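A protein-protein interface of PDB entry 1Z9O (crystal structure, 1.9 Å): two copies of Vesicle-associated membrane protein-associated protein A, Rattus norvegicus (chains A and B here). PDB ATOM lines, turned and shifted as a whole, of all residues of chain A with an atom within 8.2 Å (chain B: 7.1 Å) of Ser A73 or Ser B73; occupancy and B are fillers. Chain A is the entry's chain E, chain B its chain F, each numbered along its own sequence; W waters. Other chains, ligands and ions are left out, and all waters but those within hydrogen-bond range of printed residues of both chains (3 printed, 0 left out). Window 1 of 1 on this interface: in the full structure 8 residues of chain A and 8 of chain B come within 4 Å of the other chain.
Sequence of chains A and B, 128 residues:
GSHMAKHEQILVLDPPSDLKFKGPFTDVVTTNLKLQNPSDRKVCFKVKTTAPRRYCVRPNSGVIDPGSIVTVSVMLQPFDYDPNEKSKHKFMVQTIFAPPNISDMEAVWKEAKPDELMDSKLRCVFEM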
ATOM      1  N   LEU A  19     -11.284  21.213  18.575  1.00  0.00           N
ATOM      2  CA  LEU A  19     -10.017  21.640  19.170  1.00  0.00           C
ATOM      3  C   LEU A  19      -9.249  22.479  18.221  1.00  0.00           C
ATOM      4  O   LEU A  19      -8.898  22.042  17.175  1.00  0.00           O
ATOM      5  CB  LEU A  19      -9.115  20.451  19.587  1.00  0.00           C
ATOM      6  CG  LEU A  19      -9.382  19.585  20.741  1.00  0.00           C
ATOM      7  CD1 LEU A  19      -8.258  18.516  20.812  1.00  0.00           C
ATOM      8  CD2 LEU A  19      -9.531  20.393  22.062  1.00  0.00           C
ATOM      9  N   PHE A  21      -6.100  24.884  17.044  1.00  0.00           N
ATOM     10  CA  PHE A  21      -4.681  25.155  17.137  1.00  0.00           C
ATOM     11  C   PHE A  21      -4.146  26.297  16.303  1.00  0.00           C
ATOM     12  O   PHE A  21      -4.167  26.214  15.100  1.00  0.00           O
ATOM     13  CB  PHE A  21      -3.948  23.916  16.663  1.00  0.00           C
ATOM     14  CG  PHE A  21      -4.302  22.661  17.428  1.00  0.00           C
ATOM     15  CD1 PHE A  21      -5.399  21.921  17.071  1.00  0.00           C
ATOM     16  CD2 PHE A  21      -3.442  22.153  18.422  1.00  0.00           C
ATOM     17  CE1 PHE A  21      -5.734  20.760  17.717  1.00  0.00           C
ATOM     18  CE2 PHE A  21      -3.743  21.003  19.090  1.00  0.00           C
ATOM     19  CZ  PHE A  21      -4.931  20.266  18.731  1.00  0.00           C
ATOM     20  N   VAL A  28       6.033  23.456  18.576  1.00  0.00           N
ATOM     21  CA  VAL A  28       4.882  22.750  19.159  1.00  0.00           C
ATOM     22  C   VAL A  28       3.832  23.815  19.567  1.00  0.00           C
ATOM     23  O   VAL A  28       4.174  24.878  20.017  1.00  0.00           O
ATOM     24  CB  VAL A  28       5.298  21.905  20.474  1.00  0.00           C
ATOM     25  CG1 VAL A  28       4.073  21.351  21.153  1.00  0.00           C
ATOM     26  CG2 VAL A  28       6.270  20.812  20.121  1.00  0.00           C
ATOM     27  N   VAL A  29       2.591  23.507  19.267  1.00  0.00           N
ATOM     28  CA  VAL A  29       1.451  24.301  19.555  1.00  0.00           C
ATOM     29  C   VAL A  29       0.525  23.467  20.461  1.00  0.00           C
ATOM     30  O   VAL A  29       0.109  22.409  20.131  1.00  0.00           O
ATOM     31  CB  VAL A  29       0.789  24.741  18.187  1.00  0.00           C
ATOM     32  CG1 VAL A  29      -0.446  25.459  18.475  1.00  0.00           C
ATOM     33  CG2 VAL A  29       1.778  25.609  17.391  1.00  0.00           C
ATOM     34  N   THR A  30       0.215  23.988  21.635  1.00  0.00           N
ATOM     35  CA  THR A  30      -0.649  23.311  22.560  1.00  0.00           C
ATOM     36  C   THR A  30      -2.017  23.940  22.557  1.00  0.00           C
ATOM     37  O   THR A  30      -2.164  25.200  22.511  1.00  0.00           O
ATOM     38  CB  THR A  30       0.027  23.444  23.938  1.00  0.00           C
ATOM     39  OG1 THR A  30       1.422  23.058  23.767  1.00  0.00           O
ATOM     40  CG2 THR A  30      -0.693  22.591  25.048  1.00  0.00           C
ATOM     41  N   THR A  31      -3.017  23.109  22.642  1.00  0.00           N
ATOM     42  CA  THR A  31      -4.388  23.488  22.989  1.00  0.00           C
ATOM     43  C   THR A  31      -4.887  22.697  24.202  1.00  0.00           C
ATOM     44  O   THR A  31      -4.420  21.608  24.464  1.00  0.00           O
ATOM     45  CB  THR A  31      -5.343  23.311  21.840  1.00  0.00           C
ATOM     46  OG1 THR A  31      -4.769  23.987  20.742  1.00  0.00           O
ATOM     47  CG2 THR A  31      -6.634  24.076  22.104  1.00  0.00           C
ATOM     48  N   ASN A  32      -5.762  23.305  24.988  1.00  0.00           N
ATOM     49  CA  ASN A  32      -6.231  22.664  26.210  1.00  0.00           C
ATOM     50  C   ASN A  32      -7.650  22.152  26.099  1.00  0.00           C
ATOM     51  O   ASN A  32      -8.473  22.741  25.410  1.00  0.00           O
ATOM     52  CB  ASN A  32      -6.045  23.590  27.381  1.00  0.00           C
ATOM     53  CG  ASN A  32      -4.560  23.776  27.686  1.00  0.00           C
ATOM     54  OD1 ASN A  32      -3.788  22.763  27.890  1.00  0.00           O
ATOM     55  ND2 ASN A  32      -4.122  25.034  27.568  1.00  0.00           N
ATOM     56  N   LEU A  33      -7.846  20.987  26.681  1.00  0.00           N
ATOM     57  CA  LEU A  33      -9.090  20.369  26.801  1.00  0.00           C
ATOM     58  C   LEU A  33      -9.468  20.163  28.276  1.00  0.00           C
ATOM     59  O   LEU A  33      -8.793  19.412  28.995  1.00  0.00           O
ATOM     60  CB  LEU A  33      -9.096  19.091  25.984  1.00  0.00           C
ATOM     61  CG  LEU A  33     -10.451  18.368  26.152  1.00  0.00           C
ATOM     62  CD1 LEU A  33     -11.761  19.161  25.749  1.00  0.00           C
ATOM     63  CD2 LEU A  33     -10.229  17.039  25.419  1.00  0.00           C
ATOM     64  N   LYS A  34     -10.500  20.911  28.712  1.00  0.00           N
ATOM     65  CA  LYS A  34     -11.054  20.844  30.065  1.00  0.00           C
ATOM     66  C   LYS A  34     -12.078  19.655  30.148  1.00  0.00           C
ATOM     67  O   LYS A  34     -13.047  19.568  29.358  1.00  0.00           O
ATOM     68  CB  LYS A  34     -11.734  22.169  30.456  1.00  0.00           C
ATOM     69  CG  LYS A  34     -10.818  23.196  30.883  1.00  0.00           C
ATOM     70  CD  LYS A  34     -11.534  24.416  31.402  1.00  0.00           C
ATOM     71  CE  LYS A  34     -10.565  25.246  32.288  1.00  0.00           C
ATOM     72  NZ  LYS A  34      -9.060  25.021  31.985  1.00  0.00           N
ATOM     73  N   VAL A  47      -7.690   9.081  26.198  1.00  0.00           N
ATOM     74  CA  VAL A  47      -7.714   9.902  24.983  1.00  0.00           C
ATOM     75  C   VAL A  47      -7.046   9.024  23.795  1.00  0.00           C
ATOM     76  O   VAL A  47      -6.052   8.365  23.948  1.00  0.00           O
ATOM     77  CB  VAL A  47      -6.949  11.184  25.172  1.00  0.00           C
ATOM     78  CG1 VAL A  47      -7.132  12.002  23.990  1.00  0.00           C
ATOM     79  CG2 VAL A  47      -7.413  11.865  26.374  1.00  0.00           C
ATOM     80  N   TYR A  55       0.810  14.117  17.680  1.00  0.00           N
ATOM     81  CA  TYR A  55       0.418  14.763  18.884  1.00  0.00           C
ATOM     82  C   TYR A  55       1.047  14.045  20.094  1.00  0.00           C
ATOM     83  O   TYR A  55       1.350  12.831  20.053  1.00  0.00           O
ATOM     84  CB  TYR A  55      -1.119  14.640  19.107  1.00  0.00           C
ATOM     85  CG  TYR A  55      -1.959  15.341  18.135  1.00  0.00           C
ATOM     86  CD1 TYR A  55      -2.164  16.720  18.256  1.00  0.00           C
ATOM     87  CD2 TYR A  55      -2.443  14.721  17.033  1.00  0.00           C
ATOM     88  CE1 TYR A  55      -2.808  17.407  17.350  1.00  0.00           C
ATOM     89  CE2 TYR A  55      -3.218  15.459  16.099  1.00  0.00           C
ATOM     90  CZ  TYR A  55      -3.338  16.808  16.258  1.00  0.00           C
ATOM     91  OH  TYR A  55      -4.059  17.553  15.344  1.00  0.00           O
ATOM     92  N   CYS A  56       1.345  14.839  21.132  1.00  0.00           N
ATOM     93  CA  CYS A  56       1.540  14.350  22.524  1.00  0.00           C
ATOM     94  C   CYS A  56       0.337  14.829  23.338  1.00  0.00           C
ATOM     95  O   CYS A  56      -0.111  15.989  23.159  1.00  0.00           O
ATOM     96  CB  CYS A  56       2.833  14.848  23.173  1.00  0.00           C
ATOM     97  SG  CYS A  56       4.362  14.214  22.433  1.00  0.00           S
ATOM     98  N   VAL A  57      -0.195  13.966  24.207  1.00  0.00           N
ATOM     99  CA  VAL A  57      -1.358  14.330  24.997  1.00  0.00           C
ATOM    100  C   VAL A  57      -1.030  14.053  26.434  1.00  0.00           C
ATOM    101  O   VAL A  57      -0.629  12.926  26.793  1.00  0.00           O
ATOM    102  CB  VAL A  57      -2.603  13.522  24.535  1.00  0.00           C
ATOM    103  CG1 VAL A  57      -3.764  13.770  25.396  1.00  0.00           C
ATOM    104  CG2 VAL A  57      -2.844  13.818  23.071  1.00  0.00           C
ATOM    105  N   ARG A  58      -1.139  15.076  27.296  1.00  0.00           N
ATOM    106  CA  ARG A  58      -0.675  14.900  28.664  1.00  0.00           C
ATOM    107  C   ARG A  58      -1.734  15.518  29.641  1.00  0.00           C
ATOM    108  O   ARG A  58      -2.023  16.719  29.567  1.00  0.00           O
ATOM    109  CB  ARG A  58       0.620  15.626  28.835  1.00  0.00           C
ATOM    110  CG  ARG A  58       1.827  14.979  28.089  1.00  0.00           C
ATOM    111  CD  ARG A  58       3.021  15.739  28.240  1.00  0.00           C
ATOM    112  NE  ARG A  58       4.017  15.210  27.322  1.00  0.00           N
ATOM    113  CZ  ARG A  58       5.115  15.815  26.949  1.00  0.00           C
ATOM    114  NH1 ARG A  58       5.989  15.162  26.174  1.00  0.00           N
ATOM    115  NH2 ARG A  58       5.362  17.046  27.344  1.00  0.00           N
ATOM    116  N   PRO A  59      -2.354  14.688  30.482  1.00  0.00           N
ATOM    117  CA  PRO A  59      -2.200  13.202  30.594  1.00  0.00           C
ATOM    118  C   PRO A  59      -3.033  12.571  29.428  1.00  0.00           C
ATOM    119  O   PRO A  59      -3.957  13.204  28.903  1.00  0.00           O
ATOM    120  CB  PRO A  59      -2.803  12.910  31.957  1.00  0.00           C
ATOM    121  CG  PRO A  59      -3.830  13.900  32.075  1.00  0.00           C
ATOM    122  CD  PRO A  59      -3.376  15.170  31.433  1.00  0.00           C
ATOM    123  N   ASN A  60      -2.626  11.368  29.021  1.00  0.00           N
ATOM    124  CA  ASN A  60      -3.451  10.683  27.990  1.00  0.00           C
ATOM    125  C   ASN A  60      -4.531   9.798  28.617  1.00  0.00           C
ATOM    126  O   ASN A  60      -5.335   9.161  27.898  1.00  0.00           O
ATOM    127  CB  ASN A  60      -2.548   9.897  26.993  1.00  0.00           C
ATOM    128  CG  ASN A  60      -1.696   8.831  27.623  1.00  0.00           C
ATOM    129  OD1 ASN A  60      -1.690   8.701  28.864  1.00  0.00           O
ATOM    130  ND2 ASN A  60      -0.845   8.067  26.822  1.00  0.00           N
ATOM    131  N   VAL A  70     -10.073  18.300  35.193  1.00  0.00           N
ATOM    132  CA  VAL A  70      -8.712  18.032  34.793  1.00  0.00           C
ATOM    133  C   VAL A  70      -8.559  18.655  33.402  1.00  0.00           C
ATOM    134  O   VAL A  70      -9.469  18.475  32.516  1.00  0.00           O
ATOM    135  CB  VAL A  70      -8.435  16.511  34.733  1.00  0.00           C
ATOM    136  CG1 VAL A  70      -8.673  15.787  36.047  1.00  0.00           C
ATOM    137  CG2 VAL A  70      -9.230  15.904  33.704  1.00  0.00           C
ATOM    138  N   THR A  71      -7.467  19.411  33.186  1.00  0.00           N
ATOM    139  CA  THR A  71      -7.259  20.041  31.910  1.00  0.00           C
ATOM    140  C   THR A  71      -6.161  19.195  31.204  1.00  0.00           C
ATOM    141  O   THR A  71      -5.114  18.878  31.797  1.00  0.00           O
ATOM    142  CB  THR A  71      -6.775  21.471  31.992  1.00  0.00           C
ATOM    143  OG1 THR A  71      -7.737  22.326  32.630  1.00  0.00           O
ATOM    144  CG2 THR A  71      -6.513  21.977  30.646  1.00  0.00           C
ATOM    145  N   VAL A  72      -6.470  18.739  29.997  1.00  0.00           N
ATOM    146  CA  VAL A  72      -5.592  17.864  29.268  1.00  0.00           C
ATOM    147  C   VAL A  72      -4.881  18.765  28.270  1.00  0.00           C
ATOM    148  O   VAL A  72      -5.516  19.577  27.580  1.00  0.00           O
ATOM    149  CB  VAL A  72      -6.353  16.819  28.518  1.00  0.00           C
ATOM    150  CG1 VAL A  72      -5.476  16.137  27.454  1.00  0.00           C
ATOM    151  CG2 VAL A  72      -7.052  15.819  29.392  1.00  0.00           C
ATOM    152  N   SER A  73      -3.573  18.662  28.239  1.00  0.00           N
ATOM    153  CA  SER A  73      -2.754  19.336  27.274  1.00  0.00           C
ATOM    154  C   SER A  73      -2.540  18.531  25.934  1.00  0.00           C
ATOM    155  O   SER A  73      -2.033  17.408  25.972  1.00  0.00           O
ATOM    156  CB  SER A  73      -1.427  19.728  27.900  1.00  0.00           C
ATOM    157  OG  SER A  73      -0.710  20.366  26.919  1.00  0.00           O
ATOM    158  N   VAL A  74      -2.927  19.139  24.812  1.00  0.00           N
ATOM    159  CA  VAL A  74      -2.877  18.514  23.473  1.00  0.00           C
ATOM    160  C   VAL A  74      -1.832  19.299  22.682  1.00  0.00           C
ATOM    161  O   VAL A  74      -2.023  20.497  22.447  1.00  0.00           O
ATOM    162  CB  VAL A  74      -4.303  18.342  22.796  1.00  0.00           C
ATOM    163  CG1 VAL A  74      -4.231  17.624  21.526  1.00  0.00           C
ATOM    164  CG2 VAL A  74      -5.255  17.613  23.721  1.00  0.00           C
ATOM    165  N   MET A  75      -0.712  18.660  22.408  1.00  0.00           N
ATOM    166  CA  MET A  75       0.492  19.193  21.856  1.00  0.00           C
ATOM    167  C   MET A  75       0.709  18.703  20.433  1.00  0.00           C
ATOM    168  O   MET A  75       1.113  17.570  20.123  1.00  0.00           O
ATOM    169  CB  MET A  75       1.692  18.880  22.749  1.00  0.00           C
ATOM    170  CG  MET A  75       1.843  19.804  24.020  1.00  0.00           C
ATOM    171  SD  MET A  75       2.762  18.805  25.232  1.00  0.00           S
ATOM    172  CE  MET A  75       1.261  18.049  25.840  1.00  0.00           C
ATOM    173  N   LEU A  76       0.309  19.583  19.519  1.00  0.00           N
ATOM    174  CA  LEU A  76       0.568  19.395  18.109  1.00  0.00           C
ATOM    175  C   LEU A  76       2.044  19.578  17.765  1.00  0.00           C
ATOM    176  O   LEU A  76       2.614  20.700  17.829  1.00  0.00           O
ATOM    177  CB  LEU A  76      -0.369  20.332  17.319  1.00  0.00           C
ATOM    178  CG  LEU A  76      -0.298  20.222  15.813  1.00  0.00           C
ATOM    179  CD1 LEU A  76      -0.721  18.848  15.211  1.00  0.00           C
ATOM    180  CD2 LEU A  76      -1.095  21.422  15.245  1.00  0.00           C
ATOM    181  N   PHE A  91     -10.036  13.504  17.676  1.00  0.00           N
ATOM    182  CA  PHE A  91      -9.784  12.901  18.985  1.00  0.00           C
ATOM    183  C   PHE A  91     -11.104  12.312  19.541  1.00  0.00           C
ATOM    184  O   PHE A  91     -12.182  12.729  19.170  1.00  0.00           O
ATOM    185  CB  PHE A  91      -9.309  14.048  19.913  1.00  0.00           C
ATOM    186  CG  PHE A  91      -7.845  14.289  19.888  1.00  0.00           C
ATOM    187  CD1 PHE A  91      -7.241  15.113  18.910  1.00  0.00           C
ATOM    188  CD2 PHE A  91      -7.050  13.801  20.871  1.00  0.00           C
ATOM    189  CE1 PHE A  91      -5.815  15.316  18.938  1.00  0.00           C
ATOM    190  CE2 PHE A  91      -5.625  13.980  20.820  1.00  0.00           C
ATOM    191  CZ  PHE A  91      -5.062  14.704  19.881  1.00  0.00           C
ATOM    192  N   THR B  30       0.934  27.820  27.720  1.00  0.00           N
ATOM    193  CA  THR B  30       1.949  26.812  27.796  1.00  0.00           C
ATOM    194  C   THR B  30       3.215  27.286  27.114  1.00  0.00           C
ATOM    195  O   THR B  30       3.162  27.945  26.030  1.00  0.00           O
ATOM    196  CB  THR B  30       1.388  25.542  27.109  1.00  0.00           C
ATOM    197  OG1 THR B  30       0.086  25.238  27.692  1.00  0.00           O
ATOM    198  CG2 THR B  30       2.302  24.334  27.249  1.00  0.00           C
ATOM    199  N   THR B  31       4.336  26.989  27.714  1.00  0.00           N
ATOM    200  CA  THR B  31       5.646  27.042  27.089  1.00  0.00           C
ATOM    201  C   THR B  31       6.371  25.735  27.210  1.00  0.00           C
ATOM    202  O   THR B  31       6.144  24.961  28.139  1.00  0.00           O
ATOM    203  CB  THR B  31       6.517  28.188  27.617  1.00  0.00           C
ATOM    204  OG1 THR B  31       5.718  29.339  27.576  1.00  0.00           O
ATOM    205  CG2 THR B  31       7.622  28.548  26.594  1.00  0.00           C
ATOM    206  N   ASN B  32       7.196  25.460  26.222  1.00  0.00           N
ATOM    207  CA  ASN B  32       7.898  24.185  26.118  1.00  0.00           C
ATOM    208  C   ASN B  32       9.366  24.271  26.523  1.00  0.00           C
ATOM    209  O   ASN B  32      10.038  25.257  26.273  1.00  0.00           O
ATOM    210  CB  ASN B  32       7.719  23.617  24.753  1.00  0.00           C
ATOM    211  CG  ASN B  32       6.276  23.105  24.541  1.00  0.00           C
ATOM    212  OD1 ASN B  32       5.672  22.345  25.393  1.00  0.00           O
ATOM    213  ND2 ASN B  32       5.688  23.586  23.434  1.00  0.00           N
ATOM    214  N   LEU B  33       9.786  23.285  27.276  1.00  0.00           N
ATOM    215  CA  LEU B  33      11.137  23.139  27.643  1.00  0.00           C
ATOM    216  C   LEU B  33      11.676  21.842  27.063  1.00  0.00           C
ATOM    217  O   LEU B  33      11.191  20.740  27.399  1.00  0.00           O
ATOM    218  CB  LEU B  33      11.323  23.309  29.139  1.00  0.00           C
ATOM    219  CG  LEU B  33      12.790  23.042  29.564  1.00  0.00           C
ATOM    220  CD1 LEU B  33      13.850  23.964  28.970  1.00  0.00           C
ATOM    221  CD2 LEU B  33      12.769  22.997  31.096  1.00  0.00           C
ATOM    222  N   CYS B  56       1.265  23.937  36.124  1.00  0.00           N
ATOM    223  CA  CYS B  56       1.274  22.472  35.931  1.00  0.00           C
ATOM    224  C   CYS B  56       2.467  22.161  35.002  1.00  0.00           C
ATOM    225  O   CYS B  56       2.659  22.852  33.977  1.00  0.00           O
ATOM    226  CB  CYS B  56      -0.016  21.933  35.311  1.00  0.00           C
ATOM    227  SG  CYS B  56      -1.458  22.040  36.345  1.00  0.00           S
ATOM    228  N   VAL B  57       3.225  21.116  35.325  1.00  0.00           N
ATOM    229  CA  VAL B  57       4.356  20.730  34.505  1.00  0.00           C
ATOM    230  C   VAL B  57       4.211  19.288  34.113  1.00  0.00           C
ATOM    231  O   VAL B  57       4.109  18.425  34.982  1.00  0.00           O
ATOM    232  CB  VAL B  57       5.663  20.978  35.261  1.00  0.00           C
ATOM    233  CG1 VAL B  57       6.858  20.532  34.493  1.00  0.00           C
ATOM    234  CG2 VAL B  57       5.619  22.459  35.672  1.00  0.00           C
ATOM    235  N   ARG B  58       4.231  19.034  32.795  1.00  0.00           N
ATOM    236  CA  ARG B  58       3.949  17.652  32.357  1.00  0.00           C
ATOM    237  C   ARG B  58       4.990  17.265  31.247  1.00  0.00           C
ATOM    238  O   ARG B  58       5.038  17.957  30.212  1.00  0.00           O
ATOM    239  CB  ARG B  58       2.573  17.616  31.776  1.00  0.00           C
ATOM    240  CG  ARG B  58       1.448  17.840  32.813  1.00  0.00           C
ATOM    241  CD  ARG B  58       0.151  17.768  32.167  1.00  0.00           C
ATOM    242  NE  ARG B  58      -0.868  18.140  33.195  1.00  0.00           N
ATOM    243  CZ  ARG B  58      -2.074  18.561  32.941  1.00  0.00           C
ATOM    244  NH1 ARG B  58      -2.938  18.800  33.961  1.00  0.00           N
ATOM    245  NH2 ARG B  58      -2.468  18.684  31.683  1.00  0.00           N
ATOM    246  N   PRO B  59       5.854  16.252  31.476  1.00  0.00           N
ATOM    247  CA  PRO B  59       5.985  15.444  32.754  1.00  0.00           C
ATOM    248  C   PRO B  59       6.773  16.326  33.799  1.00  0.00           C
ATOM    249  O   PRO B  59       7.528  17.225  33.400  1.00  0.00           O
ATOM    250  CB  PRO B  59       6.762  14.217  32.299  1.00  0.00           C
ATOM    251  CG  PRO B  59       7.612  14.756  31.200  1.00  0.00           C
ATOM    252  CD  PRO B  59       6.783  15.768  30.452  1.00  0.00           C
ATOM    253  N   ASN B  60       6.484  16.110  35.094  1.00  0.00           N
ATOM    254  CA  ASN B  60       7.297  16.775  36.094  1.00  0.00           C
ATOM    255  C   ASN B  60       8.566  16.040  36.489  1.00  0.00           C
ATOM    256  O   ASN B  60       9.430  16.531  37.272  1.00  0.00           O
ATOM    257  CB  ASN B  60       6.437  17.132  37.319  1.00  0.00           C
ATOM    258  CG  ASN B  60       5.835  15.992  38.021  1.00  0.00           C
ATOM    259  OD1 ASN B  60       6.057  14.846  37.643  1.00  0.00           O
ATOM    260  ND2 ASN B  60       5.007  16.266  39.126  1.00  0.00           N
ATOM    261  N   THR B  71      10.347  16.828  25.589  1.00  0.00           N
ATOM    262  CA  THR B  71       9.885  18.209  25.685  1.00  0.00           C
ATOM    263  C   THR B  71       8.871  18.300  26.834  1.00  0.00           C
ATOM    264  O   THR B  71       7.828  17.596  26.832  1.00  0.00           O
ATOM    265  CB  THR B  71       9.156  18.739  24.477  1.00  0.00           C
ATOM    266  OG1 THR B  71      10.005  18.814  23.322  1.00  0.00           O
ATOM    267  CG2 THR B  71       8.674  20.031  24.759  1.00  0.00           C
ATOM    268  N   VAL B  72       9.162  19.165  27.784  1.00  0.00           N
ATOM    269  CA  VAL B  72       8.348  19.311  29.002  1.00  0.00           C
ATOM    270  C   VAL B  72       7.358  20.455  28.726  1.00  0.00           C
ATOM    271  O   VAL B  72       7.754  21.538  28.256  1.00  0.00           O
ATOM    272  CB  VAL B  72       9.222  19.608  30.198  1.00  0.00           C
ATOM    273  CG1 VAL B  72       8.390  19.923  31.403  1.00  0.00           C
ATOM    274  CG2 VAL B  72      10.109  18.504  30.537  1.00  0.00           C
ATOM    275  N   SER B  73       6.073  20.222  29.024  1.00  0.00           N
ATOM    276  CA  SER B  73       5.084  21.211  28.906  1.00  0.00           C
ATOM    277  C   SER B  73       4.877  21.995  30.248  1.00  0.00           C
ATOM    278  O   SER B  73       4.608  21.400  31.271  1.00  0.00           O
ATOM    279  CB  SER B  73       3.797  20.561  28.368  1.00  0.00           C
ATOM    280  OG  SER B  73       2.839  21.526  28.179  1.00  0.00           O
ATOM    281  N   VAL B  74       5.002  23.316  30.199  1.00  0.00           N
ATOM    282  CA  VAL B  74       4.931  24.175  31.409  1.00  0.00           C
ATOM    283  C   VAL B  74       3.719  25.054  31.189  1.00  0.00           C
ATOM    284  O   VAL B  74       3.724  25.872  30.230  1.00  0.00           O
ATOM    285  CB  VAL B  74       6.311  24.967  31.721  1.00  0.00           C
ATOM    286  CG1 VAL B  74       6.180  25.758  32.957  1.00  0.00           C
ATOM    287  CG2 VAL B  74       7.531  23.982  31.855  1.00  0.00           C
ATOM    288  N   MET B  75       2.700  24.847  31.995  1.00  0.00           N
ATOM    289  CA  MET B  75       1.362  25.401  31.889  1.00  0.00           C
ATOM    290  C   MET B  75       1.072  26.385  32.974  1.00  0.00           C
ATOM    291  O   MET B  75       0.874  26.066  34.164  1.00  0.00           O
ATOM    292  CB  MET B  75       0.319  24.265  31.891  1.00  0.00           C
ATOM    293  CG  MET B  75       0.160  23.528  30.540  1.00  0.00           C
ATOM    294  SD  MET B  75      -0.393  21.847  31.035  1.00  0.00           S
ATOM    295  CE  MET B  75       1.269  21.249  30.935  1.00  0.00           C
HETATM  296  O   HOH W   1       8.801  14.820  24.525  1.00  0.00           O
HETATM  297  O   HOH W   2       3.116  25.089  23.113  1.00  0.00           O
HETATM  298  O   HOH W   3      -5.516  19.168  35.538  1.00  0.00           O
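The backbone carbonyl oxygen (O) of Thr A71 is in hydrogen-bond range of the guanidinium group (NH2) of Arg B58, at 2.7 Å.
The guanidinium group of Arg A58 sits at hydrogen-bond distance from the backbone carbonyl oxygen of Thr B71 (2.6 Å).
The backbone carbonyl oxygen (O) of Arg A58 is in hydrogen-bond range of the guanidinium group (NH2) of Arg B58, 2.9 Å away.
O of Arg A58 lies within hydrogen-bond range of N of Ser A73.
The backbone carbonyl oxygen of Cys A56 lies within hydrogen-bond range of the backbone NH of Met A75.
O of Arg B58 sits at hydrogen-bond distance from N of Ser B73 (2.8 Å).
The side-chain sulfur (SD) of Met A75 lies within hydrogen-bond range of the guanidinium group (NH2) of Arg A58, at 3.8 Å.
The backbone carbonyl oxygen (O) of Cys B56 is in hydrogen-bond range of the backbone NH (N) of Met B75, at 2.8 Å.
NZ of Lys A34 lies within hydrogen-bond range of OG1 of Thr A71 (3.1 Å).
CB of Val A28 touches ND2 of Asn B32, at 3.4 Å.
CG2 of Thr B30 touches OG1 of Thr A30 (3.8 Å).
Pro B59 touches Arg A58.
Ser B73 touches Arg A58 (N to NH2, 3.7 Å).
Pro A59 touches Arg B58.
Ser A73 touches Arg B58.
Ser B73 touches Ser A73.
Ser A73 touches Met B75 (CB to SD, 3.9 Å).
Met A75 touches Ser B73.
Of chain B, only Arg B58 (3.6 Å), Ser B73 (3.9 Å) and Met B75 (3.9 Å) come within 4 Å of Ser A73.
Printed residues of chain A within 4 Å of Ser B73: Arg A58, Ser A73 and Met A75.
Printed residues of chain B within 4 Å of Arg A58: Arg B58, Pro B59, Thr B71 and Ser B73.
Printed residues of chain B within 4 Å of Thr A71: Arg B58.
Of the printed residues of chain B, Val A28 touches Asn B32 (3.4 Å).
Printed residues of chain A within 4 Å of Asn B32: Val A28 (3.4 Å).
Of the printed residues of chain A, Pro B59 touches Arg A58 (3.6 Å).
Val A57 touches none of the printed residues of chain B.
Thr A31 touches none of the printed residues of chain B.
The nearest residue of chain B that does not touch Ser A73 is Thr B30 (5.0 Å).
The nearest residue of chain A that does not touch Ser B73 is Thr A30 (4.8 Å).
Printed residues of chain A that touch a printed residue of chain B: Val A28, Thr A30, Arg A58, Pro A59, Thr A71, Ser A73 and Met A75.
Hydrophobic or aromatic side chains of chain B within 4 Å of the printed part of chain A: Pro B59 and Met B75.
Along chain B the printed residues that touch a printed residue of chain A span positions 30 to 75.
Among the printed residues, 12 pairs touch across the chains.
Thr A30 touches its own counterpart, Thr B30.
Arg A58 touches Pro B59, and with the chains exchanged Pro A59 touches Arg B58.
Arg A58 touches Thr B71, and with the chains exchanged Thr A71 touches Arg B58.
Ser B73 touches its own counterpart, Ser A73.
Of the 12 pairs that touch across the chains among the printed residues, 11 have their exchanged pair printed and touching as well.
Water W2 lies within hydrogen-bond range of OG1 of Thr A30 (2.7 Å), ND2 of Asn B32 (3.0 Å) and O of Val A28 (3.3 Å).
Water W1 bridges N of Thr B71 and NH1 of Arg A58.
Water W3 bridges the guanidinium group (NH1) of Arg B58 (3.0 Å) and the backbone NH (N) of Thr A71 (3.1 Å).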
